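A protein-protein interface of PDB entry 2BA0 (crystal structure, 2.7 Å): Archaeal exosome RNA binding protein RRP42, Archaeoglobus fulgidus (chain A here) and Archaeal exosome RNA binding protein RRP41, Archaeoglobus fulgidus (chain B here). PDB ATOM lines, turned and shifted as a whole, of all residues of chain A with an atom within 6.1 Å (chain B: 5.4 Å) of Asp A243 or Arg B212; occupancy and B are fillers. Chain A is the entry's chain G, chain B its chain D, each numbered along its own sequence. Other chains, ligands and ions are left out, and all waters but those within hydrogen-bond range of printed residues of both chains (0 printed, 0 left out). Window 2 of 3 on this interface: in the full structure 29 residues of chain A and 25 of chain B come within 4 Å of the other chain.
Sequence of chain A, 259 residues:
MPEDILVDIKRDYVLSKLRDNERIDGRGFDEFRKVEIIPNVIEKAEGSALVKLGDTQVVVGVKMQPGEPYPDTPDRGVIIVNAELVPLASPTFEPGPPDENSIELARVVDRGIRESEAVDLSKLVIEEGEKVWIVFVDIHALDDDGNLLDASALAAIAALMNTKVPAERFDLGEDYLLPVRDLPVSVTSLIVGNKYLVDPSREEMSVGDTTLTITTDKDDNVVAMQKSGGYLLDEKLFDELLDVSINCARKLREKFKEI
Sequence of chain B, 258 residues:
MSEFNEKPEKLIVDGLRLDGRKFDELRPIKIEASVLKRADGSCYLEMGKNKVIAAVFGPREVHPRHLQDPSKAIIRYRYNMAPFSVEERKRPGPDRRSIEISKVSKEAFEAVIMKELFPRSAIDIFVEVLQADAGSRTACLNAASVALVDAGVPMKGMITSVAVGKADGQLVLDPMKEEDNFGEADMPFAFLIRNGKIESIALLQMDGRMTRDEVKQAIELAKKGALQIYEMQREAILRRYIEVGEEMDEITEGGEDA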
ATOM      1  N   ILE A 214     -18.530  21.091  -3.632  1.00  0.00           N
ATOM      2  CA  ILE A 214     -19.397  21.230  -4.801  1.00  0.00           C
ATOM      3  C   ILE A 214     -20.072  22.599  -4.760  1.00  0.00           C
ATOM      4  O   ILE A 214     -20.694  22.937  -3.759  1.00  0.00           O
ATOM      5  CB  ILE A 214     -20.508  20.173  -4.793  1.00  0.00           C
ATOM      6  CG1 ILE A 214     -19.900  18.775  -4.769  1.00  0.00           C
ATOM      7  CG2 ILE A 214     -21.391  20.341  -6.002  1.00  0.00           C
ATOM      8  CD1 ILE A 214     -20.931  17.678  -4.655  1.00  0.00           C
ATOM      9  N   ASP A 220     -29.816  25.476  -9.280  1.00  0.00           N
ATOM     10  CA  ASP A 220     -29.412  24.141  -8.835  1.00  0.00           C
ATOM     11  C   ASP A 220     -28.457  23.382  -9.754  1.00  0.00           C
ATOM     12  O   ASP A 220     -28.334  22.167  -9.642  1.00  0.00           O
ATOM     13  CB  ASP A 220     -30.629  23.263  -8.576  1.00  0.00           C
ATOM     14  CG  ASP A 220     -31.352  23.633  -7.306  1.00  0.00           C
ATOM     15  OD1 ASP A 220     -30.722  24.243  -6.413  1.00  0.00           O
ATOM     16  OD2 ASP A 220     -32.552  23.293  -7.194  1.00  0.00           O
ATOM     17  N   ASN A 221     -27.784  24.086 -10.658  1.00  0.00           N
ATOM     18  CA  ASN A 221     -26.820  23.450 -11.556  1.00  0.00           C
ATOM     19  C   ASN A 221     -25.446  23.451 -10.894  1.00  0.00           C
ATOM     20  O   ASN A 221     -25.106  24.380 -10.160  1.00  0.00           O
ATOM     21  CB  ASN A 221     -26.705  24.226 -12.874  1.00  0.00           C
ATOM     22  CG  ASN A 221     -27.959  24.145 -13.723  1.00  0.00           C
ATOM     23  OD1 ASN A 221     -28.335  25.118 -14.374  1.00  0.00           O
ATOM     24  ND2 ASN A 221     -28.602  22.982 -13.734  1.00  0.00           N
ATOM     25  N   VAL A 222     -24.660  22.409 -11.142  1.00  0.00           N
ATOM     26  CA  VAL A 222     -23.311  22.360 -10.597  1.00  0.00           C
ATOM     27  C   VAL A 222     -22.514  23.334 -11.460  1.00  0.00           C
ATOM     28  O   VAL A 222     -22.703  23.396 -12.677  1.00  0.00           O
ATOM     29  CB  VAL A 222     -22.721  20.951 -10.700  1.00  0.00           C
ATOM     30  CG1 VAL A 222     -21.296  20.943 -10.195  1.00  0.00           C
ATOM     31  CG2 VAL A 222     -23.576  19.992  -9.890  1.00  0.00           C
ATOM     32  N   PHE A 238     -20.028   9.663  -3.891  1.00  0.00           N
ATOM     33  CA  PHE A 238     -20.132  10.853  -4.721  1.00  0.00           C
ATOM     34  C   PHE A 238     -21.573  11.061  -5.219  1.00  0.00           C
ATOM     35  O   PHE A 238     -22.094  12.180  -5.188  1.00  0.00           O
ATOM     36  CB  PHE A 238     -19.200  10.740  -5.924  1.00  0.00           C
ATOM     37  CG  PHE A 238     -19.296  11.898  -6.859  1.00  0.00           C
ATOM     38  CD1 PHE A 238     -18.700  13.110  -6.541  1.00  0.00           C
ATOM     39  CD2 PHE A 238     -20.018  11.798  -8.038  1.00  0.00           C
ATOM     40  CE1 PHE A 238     -18.824  14.208  -7.383  1.00  0.00           C
ATOM     41  CE2 PHE A 238     -20.149  12.896  -8.889  1.00  0.00           C
ATOM     42  CZ  PHE A 238     -19.548  14.101  -8.555  1.00  0.00           C
ATOM     43  N   ASP A 239     -22.202   9.988  -5.695  1.00  0.00           N
ATOM     44  CA  ASP A 239     -23.577  10.061  -6.185  1.00  0.00           C
ATOM     45  C   ASP A 239     -24.517  10.591  -5.107  1.00  0.00           C
ATOM     46  O   ASP A 239     -25.418  11.390  -5.380  1.00  0.00           O
ATOM     47  CB  ASP A 239     -24.065   8.677  -6.623  1.00  0.00           C
ATOM     48  CG  ASP A 239     -23.576   8.283  -8.012  1.00  0.00           C
ATOM     49  OD1 ASP A 239     -23.468   7.063  -8.260  1.00  0.00           O
ATOM     50  OD2 ASP A 239     -23.318   9.172  -8.860  1.00  0.00           O
ATOM     51  N   GLU A 240     -24.306  10.140  -3.878  1.00  0.00           N
ATOM     52  CA  GLU A 240     -25.144  10.562  -2.777  1.00  0.00           C
ATOM     53  C   GLU A 240     -24.851  12.005  -2.344  1.00  0.00           C
ATOM     54  O   GLU A 240     -25.764  12.823  -2.191  1.00  0.00           O
ATOM     55  CB  GLU A 240     -24.958   9.604  -1.603  1.00  0.00           C
ATOM     56  CG  GLU A 240     -25.816   9.921  -0.393  1.00  0.00           C
ATOM     57  CD  GLU A 240     -25.521   9.006   0.786  1.00  0.00           C
ATOM     58  OE1 GLU A 240     -25.012   7.882   0.559  1.00  0.00           O
ATOM     59  OE2 GLU A 240     -25.809   9.403   1.941  1.00  0.00           O
ATOM     60  N   LEU A 241     -23.569  12.307  -2.158  1.00  0.00           N
ATOM     61  CA  LEU A 241     -23.131  13.624  -1.722  1.00  0.00           C
ATOM     62  C   LEU A 241     -23.467  14.713  -2.737  1.00  0.00           C
ATOM     63  O   LEU A 241     -23.738  15.850  -2.375  1.00  0.00           O
ATOM     64  CB  LEU A 241     -21.626  13.589  -1.452  1.00  0.00           C
ATOM     65  CG  LEU A 241     -21.048  14.742  -0.634  1.00  0.00           C
ATOM     66  CD1 LEU A 241     -21.926  15.017   0.594  1.00  0.00           C
ATOM     67  CD2 LEU A 241     -19.624  14.384  -0.236  1.00  0.00           C
ATOM     68  N   LEU A 242     -23.451  14.364  -4.012  1.00  0.00           N
ATOM     69  CA  LEU A 242     -23.778  15.329  -5.046  1.00  0.00           C
ATOM     70  C   LEU A 242     -25.170  15.898  -4.800  1.00  0.00           C
ATOM     71  O   LEU A 242     -25.365  17.109  -4.774  1.00  0.00           O
ATOM     72  CB  LEU A 242     -23.751  14.664  -6.422  1.00  0.00           C
ATOM     73  CG  LEU A 242     -23.417  15.533  -7.635  1.00  0.00           C
ATOM     74  CD1 LEU A 242     -24.347  15.153  -8.765  1.00  0.00           C
ATOM     75  CD2 LEU A 242     -23.543  17.009  -7.303  1.00  0.00           C
ATOM     76  N   ASP A 243     -26.138  15.010  -4.626  1.00  0.00           N
ATOM     77  CA  ASP A 243     -27.516  15.413  -4.392  1.00  0.00           C
ATOM     78  C   ASP A 243     -27.685  16.078  -3.042  1.00  0.00           C
ATOM     79  O   ASP A 243     -28.356  17.099  -2.929  1.00  0.00           O
ATOM     80  CB  ASP A 243     -28.438  14.197  -4.513  1.00  0.00           C
ATOM     81  CG  ASP A 243     -28.626  13.764  -5.952  1.00  0.00           C
ATOM     82  OD1 ASP A 243     -29.516  14.334  -6.608  1.00  0.00           O
ATOM     83  OD2 ASP A 243     -27.876  12.880  -6.445  1.00  0.00           O
ATOM     84  N   VAL A 244     -27.075  15.501  -2.016  1.00  0.00           N
ATOM     85  CA  VAL A 244     -27.156  16.063  -0.682  1.00  0.00           C
ATOM     86  C   VAL A 244     -26.602  17.491  -0.744  1.00  0.00           C
ATOM     87  O   VAL A 244     -27.205  18.424  -0.215  1.00  0.00           O
ATOM     88  CB  VAL A 244     -26.352  15.185   0.312  1.00  0.00           C
ATOM     89  CG1 VAL A 244     -26.341  15.800   1.689  1.00  0.00           C
ATOM     90  CG2 VAL A 244     -26.960  13.781   0.361  1.00  0.00           C
ATOM     91  N   SER A 245     -25.472  17.657  -1.431  1.00  0.00           N
ATOM     92  CA  SER A 245     -24.829  18.958  -1.589  1.00  0.00           C
ATOM     93  C   SER A 245     -25.704  19.989  -2.296  1.00  0.00           C
ATOM     94  O   SER A 245     -25.696  21.165  -1.937  1.00  0.00           O
ATOM     95  CB  SER A 245     -23.526  18.812  -2.373  1.00  0.00           C
ATOM     96  OG  SER A 245     -22.569  18.063  -1.657  1.00  0.00           O
ATOM     97  N   ILE A 246     -26.430  19.555  -3.322  1.00  0.00           N
ATOM     98  CA  ILE A 246     -27.322  20.445  -4.064  1.00  0.00           C
ATOM     99  C   ILE A 246     -28.489  20.865  -3.160  1.00  0.00           C
ATOM    100  O   ILE A 246     -28.983  21.989  -3.261  1.00  0.00           O
ATOM    101  CB  ILE A 246     -27.869  19.749  -5.353  1.00  0.00           C
ATOM    102  CG1 ILE A 246     -26.717  19.486  -6.323  1.00  0.00           C
ATOM    103  CG2 ILE A 246     -28.921  20.613  -6.029  1.00  0.00           C
ATOM    104  CD1 ILE A 246     -27.117  18.773  -7.583  1.00  0.00           C
ATOM    105  N   ASN A 247     -28.904  19.964  -2.267  1.00  0.00           N
ATOM    106  CA  ASN A 247     -29.996  20.235  -1.330  1.00  0.00           C
ATOM    107  C   ASN A 247     -29.569  21.182  -0.204  1.00  0.00           C
ATOM    108  O   ASN A 247     -30.371  21.995   0.262  1.00  0.00           O
ATOM    109  CB  ASN A 247     -30.532  18.924  -0.724  1.00  0.00           C
ATOM    110  CG  ASN A 247     -31.497  18.186  -1.657  1.00  0.00           C
ATOM    111  N   CYS A 248     -28.314  21.059   0.238  1.00  0.00           N
ATOM    112  CA  CYS A 248     -27.753  21.912   1.294  1.00  0.00           C
ATOM    113  C   CYS A 248     -27.470  23.304   0.760  1.00  0.00           C
ATOM    114  O   CYS A 248     -27.629  24.297   1.471  1.00  0.00           O
ATOM    115  CB  CYS A 248     -26.431  21.358   1.812  1.00  0.00           C
ATOM    116  SG  CYS A 248     -26.535  19.882   2.793  1.00  0.00           S
ATOM    117  N   MET B 210     -23.255  22.613 -15.381  1.00  0.00           N
ATOM    118  CA  MET B 210     -23.754  21.295 -15.736  1.00  0.00           C
ATOM    119  C   MET B 210     -24.948  20.959 -14.876  1.00  0.00           C
ATOM    120  O   MET B 210     -25.122  21.519 -13.801  1.00  0.00           O
ATOM    121  CB  MET B 210     -22.684  20.225 -15.505  1.00  0.00           C
ATOM    122  CG  MET B 210     -21.531  20.214 -16.493  1.00  0.00           C
ATOM    123  SD  MET B 210     -20.622  18.645 -16.381  1.00  0.00           S
ATOM    124  CE  MET B 210     -19.203  18.947 -17.461  1.00  0.00           C
ATOM    125  N   THR B 211     -25.781  20.050 -15.353  1.00  0.00           N
ATOM    126  CA  THR B 211     -26.921  19.645 -14.562  1.00  0.00           C
ATOM    127  C   THR B 211     -26.480  18.411 -13.780  1.00  0.00           C
ATOM    128  O   THR B 211     -25.500  17.748 -14.139  1.00  0.00           O
ATOM    129  CB  THR B 211     -28.165  19.314 -15.440  1.00  0.00           C
ATOM    130  OG1 THR B 211     -27.863  18.229 -16.323  1.00  0.00           O
ATOM    131  CG2 THR B 211     -28.590  20.542 -16.255  1.00  0.00           C
ATOM    132  N   ARG B 212     -27.187  18.136 -12.691  1.00  0.00           N
ATOM    133  CA  ARG B 212     -26.909  16.988 -11.843  1.00  0.00           C
ATOM    134  C   ARG B 212     -26.805  15.764 -12.759  1.00  0.00           C
ATOM    135  O   ARG B 212     -25.904  14.939 -12.614  1.00  0.00           O
ATOM    136  CB  ARG B 212     -28.055  16.850 -10.839  1.00  0.00           C
ATOM    137  CG  ARG B 212     -27.914  15.786  -9.785  1.00  0.00           C
ATOM    138  CD  ARG B 212     -28.523  14.469 -10.233  1.00  0.00           C
ATOM    139  NE  ARG B 212     -28.957  13.665  -9.088  1.00  0.00           N
ATOM    140  CZ  ARG B 212     -29.535  12.469  -9.175  1.00  0.00           C
ATOM    141  NH1 ARG B 212     -29.899  11.822  -8.074  1.00  0.00           N
ATOM    142  NH2 ARG B 212     -29.744  11.914 -10.362  1.00  0.00           N
ATOM    143  N   ASP B 213     -27.710  15.689 -13.733  1.00  0.00           N
ATOM    144  CA  ASP B 213     -27.763  14.586 -14.692  1.00  0.00           C
ATOM    145  C   ASP B 213     -26.581  14.532 -15.667  1.00  0.00           C
ATOM    146  O   ASP B 213     -26.147  13.452 -16.061  1.00  0.00           O
ATOM    147  CB  ASP B 213     -29.073  14.656 -15.472  1.00  0.00           C
ATOM    148  CG  ASP B 213     -30.278  14.898 -14.569  1.00  0.00           C
ATOM    149  OD1 ASP B 213     -30.370  16.011 -13.982  1.00  0.00           O
ATOM    150  OD2 ASP B 213     -31.126  13.982 -14.444  1.00  0.00           O
ATOM    151  N   GLU B 214     -26.062  15.689 -16.060  1.00  0.00           N
ATOM    152  CA  GLU B 214     -24.915  15.734 -16.963  1.00  0.00           C
ATOM    153  C   GLU B 214     -23.610  15.353 -16.233  1.00  0.00           C
ATOM    154  O   GLU B 214     -22.659  14.853 -16.837  1.00  0.00           O
ATOM    155  CB  GLU B 214     -24.775  17.136 -17.559  1.00  0.00           C
ATOM    156  CG  GLU B 214     -25.958  17.567 -18.390  1.00  0.00           C
ATOM    157  CD  GLU B 214     -25.778  18.940 -18.994  1.00  0.00           C
ATOM    158  OE1 GLU B 214     -25.790  19.931 -18.237  1.00  0.00           O
ATOM    159  OE2 GLU B 214     -25.620  19.022 -20.232  1.00  0.00           O
ATOM    160  N   VAL B 215     -23.561  15.602 -14.931  1.00  0.00           N
ATOM    161  CA  VAL B 215     -22.373  15.264 -14.161  1.00  0.00           C
ATOM    162  C   VAL B 215     -22.235  13.738 -14.085  1.00  0.00           C
ATOM    163  O   VAL B 215     -21.145  13.189 -14.295  1.00  0.00           O
ATOM    164  CB  VAL B 215     -22.450  15.871 -12.736  1.00  0.00           C
ATOM    165  CG1 VAL B 215     -21.263  15.447 -11.914  1.00  0.00           C
ATOM    166  CG2 VAL B 215     -22.493  17.379 -12.826  1.00  0.00           C
ATOM    167  N   LYS B 216     -23.345  13.052 -13.811  1.00  0.00           N
ATOM    168  CA  LYS B 216     -23.317  11.597 -13.722  1.00  0.00           C
ATOM    169  C   LYS B 216     -22.931  10.981 -15.060  1.00  0.00           C
ATOM    170  O   LYS B 216     -22.094  10.070 -15.122  1.00  0.00           O
ATOM    171  CB  LYS B 216     -24.664  11.063 -13.259  1.00  0.00           C
ATOM    172  CG  LYS B 216     -24.976  11.388 -11.813  1.00  0.00           C
ATOM    173  CD  LYS B 216     -26.127  10.542 -11.296  1.00  0.00           C
ATOM    174  CE  LYS B 216     -26.247  10.642  -9.784  1.00  0.00           C
ATOM    175  NZ  LYS B 216     -27.145   9.597  -9.215  1.00  0.00           N
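The backbone carbonyl oxygen of Met B210 lies within hydrogen-bond range of the backbone NH of Val A222 (2.8 Å). NE of Arg B212 is in salt-bridge range of OD1 of Asp A243 (2.6 Å). The side-chain amino group (NZ) of Lys B216 lies within salt-bridge range of the side-chain carboxylate (OD2) of Asp A239 (3.9 Å).
The backbone NH (N) of Thr B211 lies within hydrogen-bond range of the side-chain carboxylate (OE1) of Glu B214 (2.9 Å).
Met B210 touches Asn A221 (O to CB, 3.3 Å). Thr B211 touches Asn A221. Leu A242 touches Arg B212. Arg B212 touches Ile A246.
Of the printed residues of chain B, Asp A239 touches Lys B216. Asp A243 touches one residue of chain B. Printed residues of chain B within 4 Å of Ile A246: Arg B212. Cys A248 touches none of the printed residues of chain B. Printed residues of chain A within 4 Å of Thr B211: Asn A221 (3.5 Å). Of chain A, only Leu A242, Asp A243 and Ile A246 come within 4 Å of Arg B212. Val B215 touches none of the printed residues of chain A.
Of the 15 printed residues of chain A, 6 touch a printed residue of chain B. Among the printed residues, Asp or Glu carboxylates within 4 Å of a Lys or Arg side-chain nitrogen of the other chain: Asp A239 with Lys B216 and Asp A243 with Arg B212.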
